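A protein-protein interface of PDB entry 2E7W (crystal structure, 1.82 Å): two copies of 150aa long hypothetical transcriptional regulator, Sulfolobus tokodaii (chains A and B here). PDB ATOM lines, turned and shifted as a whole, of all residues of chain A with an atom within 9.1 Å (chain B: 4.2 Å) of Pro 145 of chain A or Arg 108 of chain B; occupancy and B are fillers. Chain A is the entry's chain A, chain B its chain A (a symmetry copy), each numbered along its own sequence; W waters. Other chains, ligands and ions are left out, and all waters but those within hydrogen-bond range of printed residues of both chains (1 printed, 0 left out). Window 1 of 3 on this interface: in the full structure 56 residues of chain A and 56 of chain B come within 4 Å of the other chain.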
ATOM      1  N   GLN A  13     -15.338   1.323 -17.998  1.00  0.00           N
ATOM      2  CA  GLN A  13     -16.269   0.260 -17.617  1.00  0.00           C
ATOM      3  C   GLN A  13     -17.091   0.676 -16.392  1.00  0.00           C
ATOM      4  O   GLN A  13     -18.179   0.150 -16.167  1.00  0.00           O
ATOM      5  CB  GLN A  13     -15.513  -1.039 -17.301  1.00  0.00           C
ATOM      6  CG  GLN A  13     -14.607  -0.932 -16.086  1.00  0.00           C
ATOM      7  CD  GLN A  13     -13.852  -2.213 -15.770  1.00  0.00           C
ATOM      8  OE1 GLN A  13     -13.009  -2.240 -14.872  1.00  0.00           O
ATOM      9  NE2 GLN A  13     -14.147  -3.274 -16.502  1.00  0.00           N
ATOM     10  N   TYR A  51     -24.037   2.577 -22.126  1.00  0.00           N
ATOM     11  CA  TYR A  51     -25.386   2.399 -21.601  1.00  0.00           C
ATOM     12  C   TYR A  51     -25.558   3.012 -20.219  1.00  0.00           C
ATOM     13  O   TYR A  51     -24.602   3.148 -19.458  1.00  0.00           O
ATOM     14  CB  TYR A  51     -25.712   0.904 -21.490  1.00  0.00           C
ATOM     15  CG  TYR A  51     -25.421   0.069 -22.729  1.00  0.00           C
ATOM     16  CD1 TYR A  51     -25.021  -1.263 -22.609  1.00  0.00           C
ATOM     17  CD2 TYR A  51     -25.584   0.591 -24.014  1.00  0.00           C
ATOM     18  CE1 TYR A  51     -24.791  -2.057 -23.734  1.00  0.00           C
ATOM     19  CE2 TYR A  51     -25.357  -0.195 -25.148  1.00  0.00           C
ATOM     20  CZ  TYR A  51     -24.961  -1.518 -24.998  1.00  0.00           C
ATOM     21  OH  TYR A  51     -24.737  -2.301 -26.109  1.00  0.00           O
ATOM     22  N   TYR A  53     -26.875   2.579 -16.542  1.00  0.00           N
ATOM     23  CA  TYR A  53     -27.185   1.440 -15.689  1.00  0.00           C
ATOM     24  C   TYR A  53     -28.423   1.774 -14.866  1.00  0.00           C
ATOM     25  O   TYR A  53     -28.364   2.577 -13.936  1.00  0.00           O
ATOM     26  CB  TYR A  53     -26.025   1.107 -14.750  1.00  0.00           C
ATOM     27  CG  TYR A  53     -26.292  -0.136 -13.931  1.00  0.00           C
ATOM     28  CD1 TYR A  53     -26.351  -1.391 -14.536  1.00  0.00           C
ATOM     29  CD2 TYR A  53     -26.547  -0.053 -12.562  1.00  0.00           C
ATOM     30  CE1 TYR A  53     -26.663  -2.533 -13.799  1.00  0.00           C
ATOM     31  CE2 TYR A  53     -26.861  -1.189 -11.816  1.00  0.00           C
ATOM     32  CZ  TYR A  53     -26.918  -2.424 -12.441  1.00  0.00           C
ATOM     33  OH  TYR A  53     -27.237  -3.548 -11.711  1.00  0.00           O
ATOM     34  N   TRP A  92     -32.833 -11.429 -21.002  1.00  0.00           N
ATOM     35  CA  TRP A  92     -31.651 -10.651 -21.361  1.00  0.00           C
ATOM     36  C   TRP A  92     -30.429 -11.522 -21.594  1.00  0.00           C
ATOM     37  O   TRP A  92     -29.462 -11.076 -22.200  1.00  0.00           O
ATOM     38  CB  TRP A  92     -31.329  -9.581 -20.302  1.00  0.00           C
ATOM     39  CG  TRP A  92     -31.015 -10.092 -18.923  1.00  0.00           C
ATOM     40  CD1 TRP A  92     -31.868 -10.160 -17.859  1.00  0.00           C
ATOM     41  CD2 TRP A  92     -29.746 -10.561 -18.451  1.00  0.00           C
ATOM     42  NE1 TRP A  92     -31.207 -10.636 -16.751  1.00  0.00           N
ATOM     43  CE2 TRP A  92     -29.904 -10.892 -17.087  1.00  0.00           C
ATOM     44  CE3 TRP A  92     -28.489 -10.735 -19.050  1.00  0.00           C
ATOM     45  CZ2 TRP A  92     -28.853 -11.385 -16.309  1.00  0.00           C
ATOM     46  CZ3 TRP A  92     -27.442 -11.227 -18.274  1.00  0.00           C
ATOM     47  CH2 TRP A  92     -27.633 -11.546 -16.919  1.00  0.00           C
ATOM     48  N   TYR A  95     -27.622 -18.604 -22.893  1.00  0.00           N
ATOM     49  CA  TYR A  95     -26.332 -19.255 -23.082  1.00  0.00           C
ATOM     50  C   TYR A  95     -26.513 -20.743 -23.315  1.00  0.00           C
ATOM     51  O   TYR A  95     -27.440 -21.339 -22.778  1.00  0.00           O
ATOM     52  CB  TYR A  95     -25.472 -19.125 -21.816  1.00  0.00           C
ATOM     53  CG  TYR A  95     -25.352 -17.739 -21.231  1.00  0.00           C
ATOM     54  CD1 TYR A  95     -26.245 -17.288 -20.255  1.00  0.00           C
ATOM     55  CD2 TYR A  95     -24.327 -16.886 -21.632  1.00  0.00           C
ATOM     56  CE1 TYR A  95     -26.112 -16.016 -19.693  1.00  0.00           C
ATOM     57  CE2 TYR A  95     -24.185 -15.616 -21.078  1.00  0.00           C
ATOM     58  CZ  TYR A  95     -25.079 -15.186 -20.110  1.00  0.00           C
ATOM     59  OH  TYR A  95     -24.936 -13.930 -19.554  1.00  0.00           O
ATOM     60  N   MET A 106     -31.595 -16.112 -18.616  1.00  0.00           N
ATOM     61  CA  MET A 106     -31.713 -15.125 -17.545  1.00  0.00           C
ATOM     62  C   MET A 106     -32.807 -14.133 -17.929  1.00  0.00           C
ATOM     63  O   MET A 106     -32.779 -13.568 -19.022  1.00  0.00           O
ATOM     64  CB  MET A 106     -30.400 -14.357 -17.389  1.00  0.00           C
ATOM     65  CG  MET A 106     -29.134 -15.177 -17.570  1.00  0.00           C
ATOM     66  SD  MET A 106     -28.670 -16.135 -16.125  1.00  0.00           S
ATOM     67  CE  MET A 106     -28.189 -14.867 -15.039  1.00  0.00           C
ATOM     68  N   ARG A 108     -36.013 -11.126 -16.301  1.00  0.00           N
ATOM     69  CA  ARG A 108     -36.514 -10.303 -15.205  1.00  0.00           C
ATOM     70  C   ARG A 108     -37.946  -9.891 -15.518  1.00  0.00           C
ATOM     71  O   ARG A 108     -38.246  -9.511 -16.650  1.00  0.00           O
ATOM     72  CB  ARG A 108     -35.692  -9.021 -15.057  1.00  0.00           C
ATOM     73  CG  ARG A 108     -34.186  -9.171 -15.000  1.00  0.00           C
ATOM     74  CD  ARG A 108     -33.596  -7.789 -14.736  1.00  0.00           C
ATOM     75  NE  ARG A 108     -32.137  -7.742 -14.769  1.00  0.00           N
ATOM     76  CZ  ARG A 108     -31.426  -7.213 -15.761  1.00  0.00           C
ATOM     77  NH1 ARG A 108     -32.036  -6.684 -16.816  1.00  0.00           N
ATOM     78  NH2 ARG A 108     -30.102  -7.198 -15.691  1.00  0.00           N
ATOM     79  N   ILE A 140     -29.630 -11.101  -4.876  1.00  0.00           N
ATOM     80  CA  ILE A 140     -28.583 -10.780  -5.832  1.00  0.00           C
ATOM     81  C   ILE A 140     -27.422 -10.264  -4.990  1.00  0.00           C
ATOM     82  O   ILE A 140     -27.450  -9.126  -4.499  1.00  0.00           O
ATOM     83  CB  ILE A 140     -29.041  -9.689  -6.829  1.00  0.00           C
ATOM     84  CG1 ILE A 140     -30.232 -10.199  -7.645  1.00  0.00           C
ATOM     85  CG2 ILE A 140     -27.893  -9.323  -7.765  1.00  0.00           C
ATOM     86  CD1 ILE A 140     -30.783  -9.190  -8.633  1.00  0.00           C
ATOM     87  N   LYS A 142     -24.351 -10.051  -6.130  1.00  0.00           N
ATOM     88  CA  LYS A 142     -23.569  -9.220  -7.034  1.00  0.00           C
ATOM     89  C   LYS A 142     -24.054  -9.363  -8.468  1.00  0.00           C
ATOM     90  O   LYS A 142     -24.388 -10.455  -8.916  1.00  0.00           O
ATOM     91  CB  LYS A 142     -22.090  -9.616  -6.968  1.00  0.00           C
ATOM     92  CG  LYS A 142     -21.167  -8.758  -7.830  1.00  0.00           C
ATOM     93  CD  LYS A 142     -19.728  -9.243  -7.733  1.00  0.00           C
ATOM     94  CE  LYS A 142     -18.774  -8.322  -8.487  1.00  0.00           C
ATOM     95  NZ  LYS A 142     -17.371  -8.795  -8.349  1.00  0.00           N
ATOM     96  N   GLU A 143     -24.112  -8.248  -9.185  1.00  0.00           N
ATOM     97  CA  GLU A 143     -24.495  -8.279 -10.587  1.00  0.00           C
ATOM     98  C   GLU A 143     -23.880  -7.063 -11.247  1.00  0.00           C
ATOM     99  O   GLU A 143     -24.496  -5.997 -11.305  1.00  0.00           O
ATOM    100  CB  GLU A 143     -26.013  -8.258 -10.776  1.00  0.00           C
ATOM    101  CG  GLU A 143     -26.402  -8.565 -12.220  1.00  0.00           C
ATOM    102  CD  GLU A 143     -27.895  -8.560 -12.451  1.00  0.00           C
ATOM    103  OE1 GLU A 143     -28.485  -7.462 -12.457  1.00  0.00           O
ATOM    104  OE2 GLU A 143     -28.479  -9.652 -12.625  1.00  0.00           O
ATOM    105  N   SER A 144     -22.653  -7.234 -11.729  1.00  0.00           N
ATOM    106  CA  SER A 144     -21.906  -6.161 -12.375  1.00  0.00           C
ATOM    107  C   SER A 144     -21.272  -6.658 -13.669  1.00  0.00           C
ATOM    108  O   SER A 144     -20.041  -6.701 -13.795  1.00  0.00           O
ATOM    109  CB  SER A 144     -20.812  -5.656 -11.433  1.00  0.00           C
ATOM    110  OG  SER A 144     -21.375  -5.150 -10.240  1.00  0.00           O
ATOM    111  N   PRO A 145     -22.104  -7.021 -14.657  1.00  0.00           N
ATOM    112  CA  PRO A 145     -21.599  -7.518 -15.939  1.00  0.00           C
ATOM    113  C   PRO A 145     -20.696  -6.531 -16.676  1.00  0.00           C
ATOM    114  O   PRO A 145     -19.903  -6.927 -17.530  1.00  0.00           O
ATOM    115  CB  PRO A 145     -22.879  -7.852 -16.710  1.00  0.00           C
ATOM    116  CG  PRO A 145     -23.876  -6.872 -16.161  1.00  0.00           C
ATOM    117  CD  PRO A 145     -23.572  -6.896 -14.677  1.00  0.00           C
ATOM    118  N   ASN A 146     -20.813  -5.252 -16.327  1.00  0.00           N
ATOM    119  CA  ASN A 146     -20.016  -4.189 -16.941  1.00  0.00           C
ATOM    120  C   ASN A 146     -18.538  -4.287 -16.585  1.00  0.00           C
ATOM    121  O   ASN A 146     -17.683  -3.746 -17.290  1.00  0.00           O
ATOM    122  CB  ASN A 146     -20.534  -2.821 -16.492  1.00  0.00           C
ATOM    123  CG  ASN A 146     -20.520  -2.665 -14.983  1.00  0.00           C
ATOM    124  OD1 ASN A 146     -21.213  -3.391 -14.270  1.00  0.00           O
ATOM    125  ND2 ASN A 146     -19.725  -1.719 -14.486  1.00  0.00           N
ATOM    126  N   ILE A 147     -18.235  -4.964 -15.482  1.00  0.00           N
ATOM    127  CA  ILE A 147     -16.854  -5.105 -15.049  1.00  0.00           C
ATOM    128  C   ILE A 147     -16.158  -6.253 -15.754  1.00  0.00           C
ATOM    129  O   ILE A 147     -16.386  -7.427 -15.446  1.00  0.00           O
ATOM    130  CB  ILE A 147     -16.766  -5.312 -13.530  1.00  0.00           C
ATOM    131  CG1 ILE A 147     -17.525  -4.191 -12.816  1.00  0.00           C
ATOM    132  CG2 ILE A 147     -15.305  -5.314 -13.090  1.00  0.00           C
ATOM    133  CD1 ILE A 147     -17.072  -2.805 -13.212  1.00  0.00           C
ATOM    134  N   VAL A 148     -15.306  -5.901 -16.710  1.00  0.00           N
ATOM    135  CA  VAL A 148     -14.570  -6.885 -17.482  1.00  0.00           C
ATOM    136  C   VAL A 148     -13.086  -6.877 -17.130  1.00  0.00           C
ATOM    137  O   VAL A 148     -12.367  -7.831 -17.418  1.00  0.00           O
ATOM    138  CB  VAL A 148     -14.745  -6.633 -18.995  1.00  0.00           C
ATOM    139  CG1 VAL A 148     -16.160  -7.022 -19.422  1.00  0.00           C
ATOM    140  CG2 VAL A 148     -14.497  -5.166 -19.315  1.00  0.00           C
ATOM    141  N   ILE A 149     -12.639  -5.795 -16.499  1.00  0.00           N
ATOM    142  CA  ILE A 149     -11.242  -5.646 -16.089  1.00  0.00           C
ATOM    143  C   ILE A 149     -11.194  -5.510 -14.568  1.00  0.00           C
ATOM    144  O   ILE A 149     -11.656  -4.513 -14.010  1.00  0.00           O
ATOM    145  CB  ILE A 149     -10.613  -4.392 -16.743  1.00  0.00           C
ATOM    146  CG1 ILE A 149     -10.649  -4.538 -18.266  1.00  0.00           C
ATOM    147  CG2 ILE A 149      -9.176  -4.205 -16.259  1.00  0.00           C
ATOM    148  CD1 ILE A 149     -10.257  -3.281 -19.017  1.00  0.00           C
ATOM    149  N   PHE A 150     -10.643  -6.517 -13.896  1.00  0.00           N
ATOM    150  CA  PHE A 150     -10.563  -6.501 -12.438  1.00  0.00           C
ATOM    151  C   PHE A 150      -9.227  -5.981 -11.915  1.00  0.00           C
ATOM    152  O   PHE A 150      -9.122  -5.779 -10.685  1.00  0.00           O
ATOM    153  CB  PHE A 150     -10.842  -7.905 -11.875  1.00  0.00           C
ATOM    154  CG  PHE A 150     -12.254  -8.385 -12.106  1.00  0.00           C
ATOM    155  CD1 PHE A 150     -12.699  -8.702 -13.389  1.00  0.00           C
ATOM    156  CD2 PHE A 150     -13.152  -8.482 -11.045  1.00  0.00           C
ATOM    157  CE1 PHE A 150     -14.016  -9.104 -13.612  1.00  0.00           C
ATOM    158  CE2 PHE A 150     -14.468  -8.883 -11.257  1.00  0.00           C
ATOM    159  CZ  PHE A 150     -14.904  -9.194 -12.545  1.00  0.00           C
ATOM    160  OXT PHE A 150      -8.302  -5.781 -12.732  1.00  0.00           O
ATOM    161  N   LEU B  61     -11.560 -12.812 -23.350  1.00  0.00           N
ATOM    162  CA  LEU B  61     -12.302 -13.511 -22.300  1.00  0.00           C
ATOM    163  C   LEU B  61     -13.043 -14.649 -22.990  1.00  0.00           C
ATOM    164  O   LEU B  61     -14.238 -14.555 -23.281  1.00  0.00           O
ATOM    165  CB  LEU B  61     -13.278 -12.551 -21.619  1.00  0.00           C
ATOM    166  CG  LEU B  61     -12.588 -11.459 -20.795  1.00  0.00           C
ATOM    167  CD1 LEU B  61     -13.607 -10.428 -20.317  1.00  0.00           C
ATOM    168  CD2 LEU B  61     -11.868 -12.093 -19.621  1.00  0.00           C
ATOM    169  N   TYR B  63     -12.985 -18.041 -21.800  1.00  0.00           N
ATOM    170  CA  TYR B  63     -13.444 -19.095 -20.895  1.00  0.00           C
ATOM    171  C   TYR B  63     -14.537 -18.536 -19.999  1.00  0.00           C
ATOM    172  O   TYR B  63     -14.253 -17.947 -18.952  1.00  0.00           O
ATOM    173  CB  TYR B  63     -12.286 -19.599 -20.038  1.00  0.00           C
ATOM    174  CG  TYR B  63     -12.296 -21.099 -19.858  1.00  0.00           C
ATOM    175  CD1 TYR B  63     -11.899 -21.941 -20.896  1.00  0.00           C
ATOM    176  CD2 TYR B  63     -12.728 -21.674 -18.664  1.00  0.00           C
ATOM    177  CE1 TYR B  63     -11.926 -23.321 -20.752  1.00  0.00           C
ATOM    178  CE2 TYR B  63     -12.763 -23.061 -18.508  1.00  0.00           C
ATOM    179  CZ  TYR B  63     -12.359 -23.875 -19.557  1.00  0.00           C
ATOM    180  OH  TYR B  63     -12.380 -25.239 -19.411  1.00  0.00           O
ATOM    181  N   ILE B  64     -15.781 -18.733 -20.421  1.00  0.00           N
ATOM    182  CA  ILE B  64     -16.954 -18.220 -19.715  1.00  0.00           C
ATOM    183  C   ILE B  64     -17.633 -19.357 -18.955  1.00  0.00           C
ATOM    184  O   ILE B  64     -17.913 -20.412 -19.527  1.00  0.00           O
ATOM    185  CB  ILE B  64     -17.930 -17.590 -20.737  1.00  0.00           C
ATOM    186  CG1 ILE B  64     -17.171 -16.593 -21.623  1.00  0.00           C
ATOM    187  CG2 ILE B  64     -19.090 -16.914 -20.028  1.00  0.00           C
ATOM    188  CD1 ILE B  64     -16.475 -15.469 -20.871  1.00  0.00           C
ATOM    189  N   GLY B  90     -12.859 -11.879 -11.587  1.00  0.00           N
ATOM    190  CA  GLY B  90     -13.472 -12.562 -12.712  1.00  0.00           C
ATOM    191  C   GLY B  90     -14.952 -12.830 -12.500  1.00  0.00           C
ATOM    192  O   GLY B  90     -15.690 -13.024 -13.465  1.00  0.00           O
ATOM    193  N   TRP B  92     -18.615 -11.783 -11.880  1.00  0.00           N
ATOM    194  CA  TRP B  92     -19.429 -10.578 -12.018  1.00  0.00           C
ATOM    195  C   TRP B  92     -20.850 -10.774 -11.517  1.00  0.00           C
ATOM    196  O   TRP B  92     -21.553  -9.803 -11.267  1.00  0.00           O
ATOM    197  CB  TRP B  92     -19.458 -10.073 -13.472  1.00  0.00           C
ATOM    198  CG  TRP B  92     -20.043 -11.018 -14.486  1.00  0.00           C
ATOM    199  CD1 TRP B  92     -19.357 -11.848 -15.324  1.00  0.00           C
ATOM    200  CD2 TRP B  92     -21.431 -11.189 -14.798  1.00  0.00           C
ATOM    201  NE1 TRP B  92     -20.231 -12.522 -16.144  1.00  0.00           N
ATOM    202  CE2 TRP B  92     -21.511 -12.139 -15.840  1.00  0.00           C
ATOM    203  CE3 TRP B  92     -22.617 -10.633 -14.294  1.00  0.00           C
ATOM    204  CZ2 TRP B  92     -22.729 -12.544 -16.393  1.00  0.00           C
ATOM    205  CZ3 TRP B  92     -23.830 -11.038 -14.845  1.00  0.00           C
ATOM    206  CH2 TRP B  92     -23.875 -11.984 -15.883  1.00  0.00           C
ATOM    207  N   ALA B 107     -18.920 -15.950 -14.180  1.00  0.00           N
ATOM    208  CA  ALA B 107     -17.560 -15.420 -14.255  1.00  0.00           C
ATOM    209  C   ALA B 107     -16.995 -15.518 -15.660  1.00  0.00           C
ATOM    210  O   ALA B 107     -17.513 -16.262 -16.502  1.00  0.00           O
ATOM    211  CB  ALA B 107     -16.654 -16.164 -13.280  1.00  0.00           C
ATOM    212  N   ARG B 108     -15.932 -14.758 -15.911  1.00  0.00           N
ATOM    213  CA  ARG B 108     -15.277 -14.753 -17.214  1.00  0.00           C
ATOM    214  C   ARG B 108     -13.769 -14.756 -17.004  1.00  0.00           C
ATOM    215  O   ARG B 108     -13.263 -14.027 -16.150  1.00  0.00           O
ATOM    216  CB  ARG B 108     -15.626 -13.487 -18.001  1.00  0.00           C
ATOM    217  CG  ARG B 108     -17.092 -13.127 -18.111  1.00  0.00           C
ATOM    218  CD  ARG B 108     -17.200 -11.911 -19.026  1.00  0.00           C
ATOM    219  NE  ARG B 108     -18.549 -11.363 -19.143  1.00  0.00           N
ATOM    220  CZ  ARG B 108     -18.951 -10.234 -18.567  1.00  0.00           C
ATOM    221  NH1 ARG B 108     -18.111  -9.523 -17.823  1.00  0.00           N
ATOM    222  NH2 ARG B 108     -20.193  -9.806 -18.748  1.00  0.00           N
ATOM    223  N   TYR B 109     -13.061 -15.558 -17.796  1.00  0.00           N
ATOM    224  CA  TYR B 109     -11.605 -15.648 -17.718  1.00  0.00           C
ATOM    225  C   TYR B 109     -11.037 -15.765 -19.126  1.00  0.00           C
ATOM    226  O   TYR B 109     -11.753 -16.090 -20.073  1.00  0.00           O
ATOM    227  CB  TYR B 109     -11.189 -16.860 -16.874  1.00  0.00           C
ATOM    228  CG  TYR B 109     -11.644 -16.733 -15.441  1.00  0.00           C
ATOM    229  CD1 TYR B 109     -11.001 -15.855 -14.563  1.00  0.00           C
ATOM    230  CD2 TYR B 109     -12.790 -17.391 -14.993  1.00  0.00           C
ATOM    231  CE1 TYR B 109     -11.492 -15.626 -13.290  1.00  0.00           C
ATOM    232  CE2 TYR B 109     -13.292 -17.163 -13.718  1.00  0.00           C
ATOM    233  CZ  TYR B 109     -12.647 -16.279 -12.874  1.00  0.00           C
ATOM    234  OH  TYR B 109     -13.181 -16.004 -11.638  1.00  0.00           O
ATOM    235  N   GLU B 143     -26.714 -11.615 -24.537  1.00  0.00           N
ATOM    236  CA  GLU B 143     -26.247 -11.130 -23.249  1.00  0.00           C
ATOM    237  C   GLU B 143     -26.355  -9.620 -23.273  1.00  0.00           C
ATOM    238  O   GLU B 143     -25.412  -8.925 -23.656  1.00  0.00           O
ATOM    239  CB  GLU B 143     -24.801 -11.540 -22.962  1.00  0.00           C
ATOM    240  CG  GLU B 143     -24.418 -11.264 -21.511  1.00  0.00           C
ATOM    241  CD  GLU B 143     -22.998 -11.660 -21.181  1.00  0.00           C
ATOM    242  OE1 GLU B 143     -22.073 -10.954 -21.628  1.00  0.00           O
ATOM    243  OE2 GLU B 143     -22.805 -12.676 -20.478  1.00  0.00           O
ATOM    244  N   PRO B 145     -27.716  -7.425 -20.423  1.00  0.00           N
ATOM    245  CA  PRO B 145     -28.249  -7.077 -19.104  1.00  0.00           C
ATOM    246  C   PRO B 145     -28.698  -5.622 -18.979  1.00  0.00           C
ATOM    247  O   PRO B 145     -29.503  -5.289 -18.110  1.00  0.00           O
ATOM    248  CB  PRO B 145     -27.096  -7.433 -18.160  1.00  0.00           C
ATOM    249  CG  PRO B 145     -25.878  -7.215 -19.009  1.00  0.00           C
ATOM    250  CD  PRO B 145     -26.296  -7.810 -20.338  1.00  0.00           C
HETATM  251  O   HOH W   1     -16.004 -10.677 -15.815  1.00  0.00           O
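The backbone carbonyl oxygen (O) of Pro 145 of chain A sits at hydrogen-bond distance from the guanidinium group (NH2) of Arg 108 of chain B, 3.1 Å away. OE2 of Glu 143 of chain B sits at hydrogen-bond distance from OH of Tyr 95 of chain A. NH2 of Arg 108 of chain A lies within hydrogen-bond range of O of Pro 145 of chain B (3.1 Å). The backbone NH of Ser 144 of chain A lies within hydrogen-bond range of the backbone carbonyl oxygen of Trp 92 of chain B (2.8 Å).
NH2 of Arg 108 of chain B is in salt-bridge range of OE1 of Glu 143 of chain B. The backbone NH of Arg 108 of chain B sits at hydrogen-bond distance from the backbone carbonyl oxygen of Gly 90 of chain B (3.0 Å). The backbone NH (N) of Trp 92 of chain A lies within hydrogen-bond range of the backbone carbonyl oxygen (O) of Met 106 of chain A (2.9 Å). NE2 of Gln 13 of chain A sits close to N of Val 148 of chain A, 2.9 Å away. The side-chain carboxylate of Glu 143 of chain A is in salt-bridge range of the guanidinium group of Arg 108 of chain A, 3.6 Å away.
Trp 92 of chain B touches Trp 92 of chain A (CH2 to CH2, 3.9 Å). O of Trp 92 of chain A touches CA of Glu 143 of chain B, at 3.4 Å. Pro 145 of chain B touches Trp 92 of chain A. Lys 142 of chain A touches Trp 92 of chain B. CA of Glu 143 of chain A touches O of Trp 92 of chain B, 3.4 Å away. Pro 145 of chain A touches Trp 92 of chain B. Pro 145 of chain B touches Pro 145 of chain A (CG to CG, 3.5 Å). O of Ile 147 of chain A touches NH1 of Arg 108 of chain B (3.6 Å). Val 148 of chain A touches Arg 108 of chain B. Phe 150 of chain A touches Gly 90 of chain B (CE2 to N, 3.4 Å).
Pro 145 of chain A touches three residues of chain B. Printed residues of chain B within 4 Å of Val 148 of chain A: Arg 108. Arg 108 of chain B touches three residues of chain A. Printed residues of chain A within 4 Å of Glu 143 of chain B: Trp 92 (3.4 Å) and Tyr 95 (2.6 Å). Of the printed residues of chain A, Pro 145 of chain B touches Trp 92, Arg 108 and Pro 145. The nearest residue of chain A that does not touch Arg 108 of chain B is Asn 146 of chain A (5.2 Å).
Of the 10 printed residues of chain B, 5 touch a printed residue of chain A. Printed residues of chain B that touch a printed residue of chain A: Gly 90, Trp 92, Arg 108, Glu 143 and Pro 145. Hydrophobic or aromatic side chains of chain B within 4 Å of the printed part of chain A: Trp 92 and Pro 145. Of the 17 printed residues of chain A, 10 touch a printed residue of chain B. Along chain A the printed residues that touch a printed residue of chain B span positions 92 to 150. Among the printed residues, 14 pairs touch across the chains. Among the printed residues, no Asp or Glu carboxylate lies within 4 Å of a Lys or Arg side-chain nitrogen of the other chain.
Trp 92 of chain A touches Glu 143 of chain B, and with the chains exchanged Glu 143 of chain A touches Trp 92 of chain B. Trp 92 of chain A touches Pro 145 of chain B, and with the chains exchanged Pro 145 of chain A touches Trp 92 of chain B. Arg 108 of chain A touches Pro 145 of chain B, and with the chains exchanged Pro 145 of chain A touches Arg 108 of chain B. Pro 145 of chain B touches its own counterpart, Pro 145 of chain A. Of the 14 pairs that touch across the chains among the printed residues, 8 have their exchanged pair printed and touching as well.
Water W1 lies within hydrogen-bond range of NH1 of Arg 108 of chain B (3.1 Å), O of Ile 147 of chain A (3.3 Å) and O of Gly 90 of chain B (3.3 Å).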
